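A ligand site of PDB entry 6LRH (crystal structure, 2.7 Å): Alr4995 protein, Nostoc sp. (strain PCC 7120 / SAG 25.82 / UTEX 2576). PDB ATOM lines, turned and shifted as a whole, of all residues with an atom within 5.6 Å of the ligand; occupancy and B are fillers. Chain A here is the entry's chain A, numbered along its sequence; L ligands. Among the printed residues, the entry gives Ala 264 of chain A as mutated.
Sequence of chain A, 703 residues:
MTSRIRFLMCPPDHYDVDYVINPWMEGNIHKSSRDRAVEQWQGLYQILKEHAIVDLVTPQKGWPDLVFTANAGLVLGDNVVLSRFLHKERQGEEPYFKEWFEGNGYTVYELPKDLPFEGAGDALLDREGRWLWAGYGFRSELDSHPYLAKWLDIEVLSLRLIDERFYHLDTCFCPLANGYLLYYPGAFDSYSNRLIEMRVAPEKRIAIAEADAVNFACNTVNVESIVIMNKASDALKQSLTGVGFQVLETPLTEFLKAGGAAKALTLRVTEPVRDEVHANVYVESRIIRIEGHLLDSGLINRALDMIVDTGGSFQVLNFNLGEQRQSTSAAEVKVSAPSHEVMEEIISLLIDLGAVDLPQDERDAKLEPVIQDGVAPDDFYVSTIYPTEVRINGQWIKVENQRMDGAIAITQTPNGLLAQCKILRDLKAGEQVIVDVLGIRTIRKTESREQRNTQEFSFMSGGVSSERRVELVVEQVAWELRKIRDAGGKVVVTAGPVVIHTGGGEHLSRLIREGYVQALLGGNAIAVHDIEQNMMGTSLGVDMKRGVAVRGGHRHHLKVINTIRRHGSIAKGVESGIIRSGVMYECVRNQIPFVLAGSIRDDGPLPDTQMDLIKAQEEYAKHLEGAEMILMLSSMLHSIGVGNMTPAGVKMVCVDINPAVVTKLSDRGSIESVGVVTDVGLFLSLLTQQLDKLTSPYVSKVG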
ATOM      1  N   TYR A  19      22.343 -15.937 -10.784  1.00  0.00           N
ATOM      2  CA  TYR A  19      23.204 -17.108 -10.659  1.00  0.00           C
ATOM      3  C   TYR A  19      24.510 -16.913 -11.435  1.00  0.00           C
ATOM      4  O   TYR A  19      24.739 -15.866 -12.021  1.00  0.00           O
ATOM      5  CB  TYR A  19      22.483 -18.347 -11.145  1.00  0.00           C
ATOM      6  CG  TYR A  19      21.712 -18.142 -12.424  1.00  0.00           C
ATOM      7  CD1 TYR A  19      22.322 -18.291 -13.655  1.00  0.00           C
ATOM      8  CD2 TYR A  19      20.371 -17.810 -12.400  1.00  0.00           C
ATOM      9  CE1 TYR A  19      21.624 -18.112 -14.814  1.00  0.00           C
ATOM     10  CE2 TYR A  19      19.664 -17.635 -13.559  1.00  0.00           C
ATOM     11  CZ  TYR A  19      20.296 -17.786 -14.770  1.00  0.00           C
ATOM     12  OH  TYR A  19      19.591 -17.595 -15.925  1.00  0.00           O
ATOM     13  N   ILE A  21      26.631 -18.945 -14.298  1.00  0.00           N
ATOM     14  CA  ILE A  21      26.839 -20.056 -15.212  1.00  0.00           C
ATOM     15  C   ILE A  21      27.747 -19.689 -16.368  1.00  0.00           C
ATOM     16  O   ILE A  21      27.801 -20.399 -17.365  1.00  0.00           O
ATOM     17  CB  ILE A  21      25.511 -20.593 -15.764  1.00  0.00           C
ATOM     18  CG1 ILE A  21      24.818 -19.547 -16.641  1.00  0.00           C
ATOM     19  CG2 ILE A  21      24.614 -21.054 -14.641  1.00  0.00           C
ATOM     20  CD1 ILE A  21      23.497 -19.984 -17.144  1.00  0.00           C
ATOM     21  N   ASN A  22      28.456 -18.569 -16.250  1.00  0.00           N
ATOM     22  CA  ASN A  22      29.558 -18.241 -17.141  1.00  0.00           C
ATOM     23  C   ASN A  22      30.438 -17.241 -16.391  1.00  0.00           C
ATOM     24  O   ASN A  22      30.031 -16.726 -15.374  1.00  0.00           O
ATOM     25  CB  ASN A  22      29.061 -17.732 -18.509  1.00  0.00           C
ATOM     26  CG  ASN A  22      28.560 -16.287 -18.479  1.00  0.00           C
ATOM     27  OD1 ASN A  22      29.297 -15.368 -18.175  1.00  0.00           O
ATOM     28  ND2 ASN A  22      27.304 -16.094 -18.870  1.00  0.00           N
ATOM     29  N   MET A  25      29.372 -13.577 -15.250  1.00  0.00           N
ATOM     30  CA  MET A  25      28.397 -13.469 -14.192  1.00  0.00           C
ATOM     31  C   MET A  25      29.059 -13.498 -12.838  1.00  0.00           C
ATOM     32  O   MET A  25      28.490 -13.016 -11.865  1.00  0.00           O
ATOM     33  CB  MET A  25      27.368 -14.579 -14.304  1.00  0.00           C
ATOM     34  CG  MET A  25      26.641 -14.564 -15.629  1.00  0.00           C
ATOM     35  SD  MET A  25      25.367 -15.819 -15.809  1.00  0.00           S
ATOM     36  CE  MET A  25      24.002 -14.983 -15.064  1.00  0.00           C
ATOM     37  N   ASP A  65      17.301 -14.721 -17.789  1.00  0.00           N
ATOM     38  CA  ASP A  65      18.043 -14.792 -19.044  1.00  0.00           C
ATOM     39  C   ASP A  65      17.148 -15.007 -20.252  1.00  0.00           C
ATOM     40  O   ASP A  65      17.618 -15.195 -21.354  1.00  0.00           O
ATOM     41  CB  ASP A  65      19.102 -15.896 -18.971  1.00  0.00           C
ATOM     42  CG  ASP A  65      20.367 -15.462 -18.231  1.00  0.00           C
ATOM     43  OD1 ASP A  65      20.774 -14.287 -18.309  1.00  0.00           O
ATOM     44  OD2 ASP A  65      20.986 -16.308 -17.545  1.00  0.00           O
ATOM     45  N   PHE A  68      17.810 -13.007 -23.459  1.00  0.00           N
ATOM     46  CA  PHE A  68      18.769 -13.395 -24.473  1.00  0.00           C
ATOM     47  C   PHE A  68      18.153 -14.375 -25.438  1.00  0.00           C
ATOM     48  O   PHE A  68      18.422 -15.567 -25.417  1.00  0.00           O
ATOM     49  CB  PHE A  68      20.026 -13.994 -23.831  1.00  0.00           C
ATOM     50  CG  PHE A  68      20.740 -13.051 -22.940  1.00  0.00           C
ATOM     51  CD1 PHE A  68      21.344 -11.924 -23.459  1.00  0.00           C
ATOM     52  CD2 PHE A  68      20.809 -13.279 -21.583  1.00  0.00           C
ATOM     53  CE1 PHE A  68      21.995 -11.039 -22.646  1.00  0.00           C
ATOM     54  CE2 PHE A  68      21.469 -12.392 -20.755  1.00  0.00           C
ATOM     55  CZ  PHE A  68      22.072 -11.278 -21.292  1.00  0.00           C
ATOM     56  N   ALA A  70      18.736 -14.894 -28.370  1.00  0.00           N
ATOM     57  CA  ALA A  70      19.667 -15.508 -29.310  1.00  0.00           C
ATOM     58  C   ALA A  70      19.820 -16.996 -29.076  1.00  0.00           C
ATOM     59  O   ALA A  70      20.200 -17.725 -29.979  1.00  0.00           O
ATOM     60  CB  ALA A  70      20.996 -14.850 -29.247  1.00  0.00           C
ATOM     61  N   ASN A  71      19.529 -17.419 -27.853  1.00  0.00           N
ATOM     62  CA  ASN A  71      19.661 -18.815 -27.483  1.00  0.00           C
ATOM     63  C   ASN A  71      18.354 -19.560 -27.497  1.00  0.00           C
ATOM     64  O   ASN A  71      18.275 -20.622 -26.931  1.00  0.00           O
ATOM     65  CB  ASN A  71      20.268 -18.976 -26.087  1.00  0.00           C
ATOM     66  CG  ASN A  71      21.548 -18.216 -25.892  1.00  0.00           C
ATOM     67  OD1 ASN A  71      21.663 -17.401 -24.987  1.00  0.00           O
ATOM     68  ND2 ASN A  71      22.536 -18.480 -26.743  1.00  0.00           N
ATOM     69  N   ARG A  90      18.512 -22.126 -17.028  1.00  0.00           N
ATOM     70  CA  ARG A  90      17.920 -21.601 -18.240  1.00  0.00           C
ATOM     71  C   ARG A  90      16.971 -22.600 -18.876  1.00  0.00           C
ATOM     72  O   ARG A  90      16.320 -22.292 -19.857  1.00  0.00           O
ATOM     73  CB  ARG A  90      19.005 -21.204 -19.251  1.00  0.00           C
ATOM     74  CG  ARG A  90      19.807 -19.986 -18.878  1.00  0.00           C
ATOM     75  CD  ARG A  90      20.423 -19.322 -20.107  1.00  0.00           C
ATOM     76  NE  ARG A  90      19.420 -18.649 -20.935  1.00  0.00           N
ATOM     77  CZ  ARG A  90      19.675 -18.018 -22.071  1.00  0.00           C
ATOM     78  NH1 ARG A  90      20.897 -17.949 -22.539  1.00  0.00           N
ATOM     79  NH2 ARG A  90      18.696 -17.454 -22.746  1.00  0.00           N
ATOM     80  N   GLU A 118      22.427 -24.485 -27.888  1.00  0.00           N
ATOM     81  CA  GLU A 118      21.859 -23.238 -27.416  1.00  0.00           C
ATOM     82  C   GLU A 118      21.607 -22.213 -28.529  1.00  0.00           C
ATOM     83  O   GLU A 118      21.705 -21.015 -28.313  1.00  0.00           O
ATOM     84  CB  GLU A 118      22.732 -22.647 -26.312  1.00  0.00           C
ATOM     85  CG  GLU A 118      23.175 -23.668 -25.281  1.00  0.00           C
ATOM     86  CD  GLU A 118      23.363 -23.102 -23.882  1.00  0.00           C
ATOM     87  OE1 GLU A 118      23.654 -21.907 -23.721  1.00  0.00           O
ATOM     88  OE2 GLU A 118      23.212 -23.864 -22.925  1.00  0.00           O
ATOM     89  N   GLY A 121      22.852 -18.254 -30.884  1.00  0.00           N
ATOM     90  CA  GLY A 121      23.977 -17.852 -30.064  1.00  0.00           C
ATOM     91  C   GLY A 121      25.180 -18.744 -30.236  1.00  0.00           C
ATOM     92  O   GLY A 121      26.285 -18.267 -30.135  1.00  0.00           O
ATOM     93  N   ARG A 139      29.016 -25.067 -24.377  1.00  0.00           N
ATOM     94  CA  ARG A 139      27.567 -25.149 -24.244  1.00  0.00           C
ATOM     95  C   ARG A 139      26.988 -26.202 -25.149  1.00  0.00           C
ATOM     96  O   ARG A 139      26.662 -27.279 -24.691  1.00  0.00           O
ATOM     97  CB  ARG A 139      26.912 -23.806 -24.525  1.00  0.00           C
ATOM     98  CG  ARG A 139      27.150 -22.769 -23.458  1.00  0.00           C
ATOM     99  CD  ARG A 139      26.579 -23.184 -22.144  1.00  0.00           C
ATOM    100  NE  ARG A 139      26.812 -22.198 -21.090  1.00  0.00           N
ATOM    101  CZ  ARG A 139      26.075 -21.112 -20.907  1.00  0.00           C
ATOM    102  NH1 ARG A 139      25.060 -20.846 -21.710  1.00  0.00           N
ATOM    103  NH2 ARG A 139      26.368 -20.278 -19.933  1.00  0.00           N
ATOM    104  N   TYR A 167      32.239 -18.275 -24.554  1.00  0.00           N
ATOM    105  CA  TYR A 167      31.617 -19.588 -24.420  1.00  0.00           C
ATOM    106  C   TYR A 167      30.507 -19.880 -25.460  1.00  0.00           C
ATOM    107  O   TYR A 167      30.177 -21.036 -25.689  1.00  0.00           O
ATOM    108  CB  TYR A 167      31.061 -19.727 -22.997  1.00  0.00           C
ATOM    109  CG  TYR A 167      30.045 -18.681 -22.677  1.00  0.00           C
ATOM    110  CD1 TYR A 167      30.413 -17.421 -22.261  1.00  0.00           C
ATOM    111  CD2 TYR A 167      28.696 -18.946 -22.840  1.00  0.00           C
ATOM    112  CE1 TYR A 167      29.481 -16.450 -22.003  1.00  0.00           C
ATOM    113  CE2 TYR A 167      27.749 -17.989 -22.591  1.00  0.00           C
ATOM    114  CZ  TYR A 167      28.137 -16.744 -22.173  1.00  0.00           C
ATOM    115  OH  TYR A 167      27.190 -15.808 -21.916  1.00  0.00           O
ATOM    116  N   HIS A 168      29.935 -18.830 -26.051  1.00  0.00           N
ATOM    117  CA  HIS A 168      29.028 -18.934 -27.199  1.00  0.00           C
ATOM    118  C   HIS A 168      29.719 -18.439 -28.426  1.00  0.00           C
ATOM    119  O   HIS A 168      30.450 -17.490 -28.347  1.00  0.00           O
ATOM    120  CB  HIS A 168      27.756 -18.105 -27.011  1.00  0.00           C
ATOM    121  CG  HIS A 168      26.728 -18.772 -26.177  1.00  0.00           C
ATOM    122  ND1 HIS A 168      25.889 -18.083 -25.332  1.00  0.00           N
ATOM    123  CD2 HIS A 168      26.390 -20.078 -26.035  1.00  0.00           C
ATOM    124  CE1 HIS A 168      25.096 -18.922 -24.704  1.00  0.00           C
ATOM    125  NE2 HIS A 168      25.375 -20.138 -25.122  1.00  0.00           N
ATOM    126  N   ASP A 170      28.717 -16.637 -30.742  1.00  0.00           N
ATOM    127  CA  ASP A 170      28.389 -15.295 -31.159  1.00  0.00           C
ATOM    128  C   ASP A 170      29.044 -14.228 -30.290  1.00  0.00           C
ATOM    129  O   ASP A 170      28.768 -13.057 -30.456  1.00  0.00           O
ATOM    130  CB  ASP A 170      26.879 -15.121 -31.204  1.00  0.00           C
ATOM    131  CG  ASP A 170      26.246 -14.875 -29.828  1.00  0.00           C
ATOM    132  OD1 ASP A 170      26.897 -15.014 -28.788  1.00  0.00           O
ATOM    133  OD2 ASP A 170      25.039 -14.555 -29.807  1.00  0.00           O
ATOM    134  N   THR A 171      29.914 -14.623 -29.375  1.00  0.00           N
ATOM    135  CA  THR A 171      30.699 -13.688 -28.570  1.00  0.00           C
ATOM    136  C   THR A 171      32.074 -13.379 -29.188  1.00  0.00           C
ATOM    137  O   THR A 171      32.768 -12.464 -28.758  1.00  0.00           O
ATOM    138  CB  THR A 171      30.916 -14.223 -27.142  1.00  0.00           C
ATOM    139  OG1 THR A 171      31.680 -15.421 -27.180  1.00  0.00           O
ATOM    140  CG2 THR A 171      29.603 -14.509 -26.477  1.00  0.00           C
ATOM    141  N   PHE A 216      32.842  -7.080 -26.296  1.00  0.00           N
ATOM    142  CA  PHE A 216      31.855  -7.856 -27.039  1.00  0.00           C
ATOM    143  C   PHE A 216      31.615  -7.327 -28.438  1.00  0.00           C
ATOM    144  O   PHE A 216      30.489  -7.362 -28.919  1.00  0.00           O
ATOM    145  CB  PHE A 216      30.521  -7.920 -26.277  1.00  0.00           C
ATOM    146  CG  PHE A 216      30.388  -9.094 -25.329  1.00  0.00           C
ATOM    147  CD1 PHE A 216      30.766  -8.985 -24.017  1.00  0.00           C
ATOM    148  CD2 PHE A 216      29.862 -10.296 -25.771  1.00  0.00           C
ATOM    149  CE1 PHE A 216      30.618 -10.057 -23.157  1.00  0.00           C
ATOM    150  CE2 PHE A 216      29.734 -11.363 -24.918  1.00  0.00           C
ATOM    151  CZ  PHE A 216      30.103 -11.254 -23.621  1.00  0.00           C
ATOM    152  N   ASN A 219      29.870  -9.552 -30.783  1.00  0.00           N
ATOM    153  CA  ASN A 219      28.459  -9.748 -30.477  1.00  0.00           C
ATOM    154  C   ASN A 219      27.627  -8.676 -31.150  1.00  0.00           C
ATOM    155  O   ASN A 219      26.930  -7.913 -30.520  1.00  0.00           O
ATOM    156  CB  ASN A 219      28.251  -9.760 -28.974  1.00  0.00           C
ATOM    157  CG  ASN A 219      27.103 -10.632 -28.554  1.00  0.00           C
ATOM    158  OD1 ASN A 219      26.286 -10.233 -27.751  1.00  0.00           O
ATOM    159  ND2 ASN A 219      27.037 -11.829 -29.110  1.00  0.00           N
ATOM    160  N   ALA A 258      25.939 -10.217 -17.405  1.00  0.00           N
ATOM    161  CA  ALA A 258      25.438 -11.583 -17.504  1.00  0.00           C
ATOM    162  C   ALA A 258      26.094 -12.349 -18.638  1.00  0.00           C
ATOM    163  O   ALA A 258      25.826 -13.518 -18.837  1.00  0.00           O
ATOM    164  CB  ALA A 258      23.944 -11.575 -17.674  1.00  0.00           C
ATOM    165  N   GLY A 259      26.947 -11.692 -19.391  1.00  0.00           N
ATOM    166  CA  GLY A 259      27.656 -12.340 -20.467  1.00  0.00           C
ATOM    167  C   GLY A 259      27.068 -12.214 -21.851  1.00  0.00           C
ATOM    168  O   GLY A 259      27.351 -13.021 -22.718  1.00  0.00           O
ATOM    169  N   GLY A 260      26.235 -11.195 -22.069  1.00  0.00           N
ATOM    170  CA  GLY A 260      25.722 -10.928 -23.398  1.00  0.00           C
ATOM    171  C   GLY A 260      25.739  -9.482 -23.807  1.00  0.00           C
ATOM    172  O   GLY A 260      25.807  -8.617 -22.966  1.00  0.00           O
ATOM    173  N   ALA A 261      25.684  -9.211 -25.109  1.00  0.00           N
ATOM    174  CA  ALA A 261      25.534  -7.862 -25.615  1.00  0.00           C
ATOM    175  C   ALA A 261      24.412  -7.770 -26.656  1.00  0.00           C
ATOM    176  O   ALA A 261      23.380  -8.397 -26.507  1.00  0.00           O
ATOM    177  CB  ALA A 261      26.827  -7.374 -26.196  1.00  0.00           C
ATOM    178  N   LYS A 263      23.954  -8.786 -30.005  1.00  0.00           N
ATOM    179  CA  LYS A 263      23.482  -9.927 -30.772  1.00  0.00           C
ATOM    180  C   LYS A 263      22.842 -10.990 -29.911  1.00  0.00           C
ATOM    181  O   LYS A 263      21.993 -11.729 -30.389  1.00  0.00           O
ATOM    182  CB  LYS A 263      24.590 -10.548 -31.585  1.00  0.00           C
ATOM    183  CG  LYS A 263      24.082 -11.500 -32.629  1.00  0.00           C
ATOM    184  CD  LYS A 263      25.185 -11.983 -33.486  1.00  0.00           C
ATOM    185  CE  LYS A 263      24.708 -12.310 -34.871  1.00  0.00           C
ATOM    186  NZ  LYS A 263      25.847 -12.065 -35.779  1.00  0.00           N
ATOM    187  N   ALA A 264      23.254 -11.092 -28.650  1.00  0.00           N
ATOM    188  CA  ALA A 264      22.658 -12.025 -27.706  1.00  0.00           C
ATOM    189  C   ALA A 264      21.203 -11.666 -27.375  1.00  0.00           C
ATOM    190  O   ALA A 264      20.422 -12.538 -27.042  1.00  0.00           O
ATOM    191  CB  ALA A 264      23.459 -12.073 -26.467  1.00  0.00           C
HETATM  192  N1  LIG L   1      23.330 -15.673 -18.857  1.00  0.00           N
HETATM  193  C1  LIG L   1      23.247 -16.206 -20.210  1.00  0.00           C
HETATM  194  C2  LIG L   1      23.912 -17.550 -20.274  1.00  0.00           C
HETATM  195  O1  LIG L   1      24.881 -17.820 -19.579  1.00  0.00           O
HETATM  196  C3  LIG L   1      23.866 -15.261 -21.232  1.00  0.00           C
HETATM  197  C4  LIG L   1      23.629 -15.697 -22.653  1.00  0.00           C
HETATM  198  C5  LIG L   1      24.401 -14.920 -23.656  1.00  0.00           C
HETATM  199  N2  LIG L   1      23.989 -15.285 -25.011  1.00  0.00           N
HETATM  200  C6  LIG L   1      24.725 -15.114 -26.091  1.00  0.00           C
HETATM  201  N3  LIG L   1      24.245 -15.471 -27.265  1.00  0.00           N
HETATM  202  N4  LIG L   1      25.930 -14.586 -26.012  1.00  0.00           N
HETATM  203  O2  LIG L   1      23.495 -18.386 -21.036  1.00  0.00           O
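The side-chain carboxylate (OD2) of Asp 65 is in salt-bridge range of a nitrogen (N1) of the ligand.
The side-chain carboxylate (OD2) of Asp 170 lies within salt-bridge range of a nitrogen (N3) of the ligand (2.8 Å).
NH2 of Arg 139 lies within salt-bridge range of O1 of the ligand.
O2 of the ligand is in salt-bridge range of NH1 of Arg 90, at 3.0 Å.
An oxygen (O1) of the ligand is in hydrogen-bond range of the side-chain amide nitrogen (ND2) of Asn 22, at 3.1 Å.
The side-chain amide oxygen (OD1) of Asn 71 is in hydrogen-bond range of a nitrogen (N2) of the ligand, at 3.1 Å.
A nitrogen (N2) of the ligand sits close to a ring nitrogen (ND1) of His 168, at 3.4 Å.
The backbone carbonyl oxygen (O) of Ala 258 sits at hydrogen-bond distance from a nitrogen (N1) of the ligand (3.3 Å).
The side-chain sulfur of Met 25 is in hydrogen-bond range of a nitrogen (N1) of the ligand (3.7 Å).
Residues that only touch the ligand: Ile 21, Phe 68, Ala 70, Gly 121, Tyr 167, Thr 171, Gly 259 and Ala 264.
Hydrophobic or aromatic side chains within 4 Å of the ligand: Ile 21, Met 25, Phe 68, Ala 70, His 168 and Ala 264.
The nearest printed residue that does not touch the ligand is Gly 260 (4.2 Å).
The side-chain hydroxyl (OH) of Tyr 19 lies within hydrogen-bond range of the side-chain carboxylate (OD2) of Asp 65, 2.5 Å away.
The guanidinium group (NH1) of Arg 139 sits at hydrogen-bond distance from a ring nitrogen (NE2) of His 168, 3.5 Å away.
The guanidinium group of Arg 139 lies within salt-bridge range of the side-chain carboxylate of Glu 118 (2.7 Å).
OD1 of Asn 71 is in hydrogen-bond range of NH1 of Arg 90, at 2.6 Å.
ND2 of Asn 22 is in hydrogen-bond range of O of Ala 258.
The backbone carbonyl oxygen (O) of Glu 118 is in hydrogen-bond range of the side-chain amide nitrogen (ND2) of Asn 71.
The backbone NH (N) of Ala 70 sits at hydrogen-bond distance from the backbone carbonyl oxygen (O) of Ala 264, at 3.2 Å.
OH of Tyr 167 lies within hydrogen-bond range of O of Gly 259 (2.9 Å).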
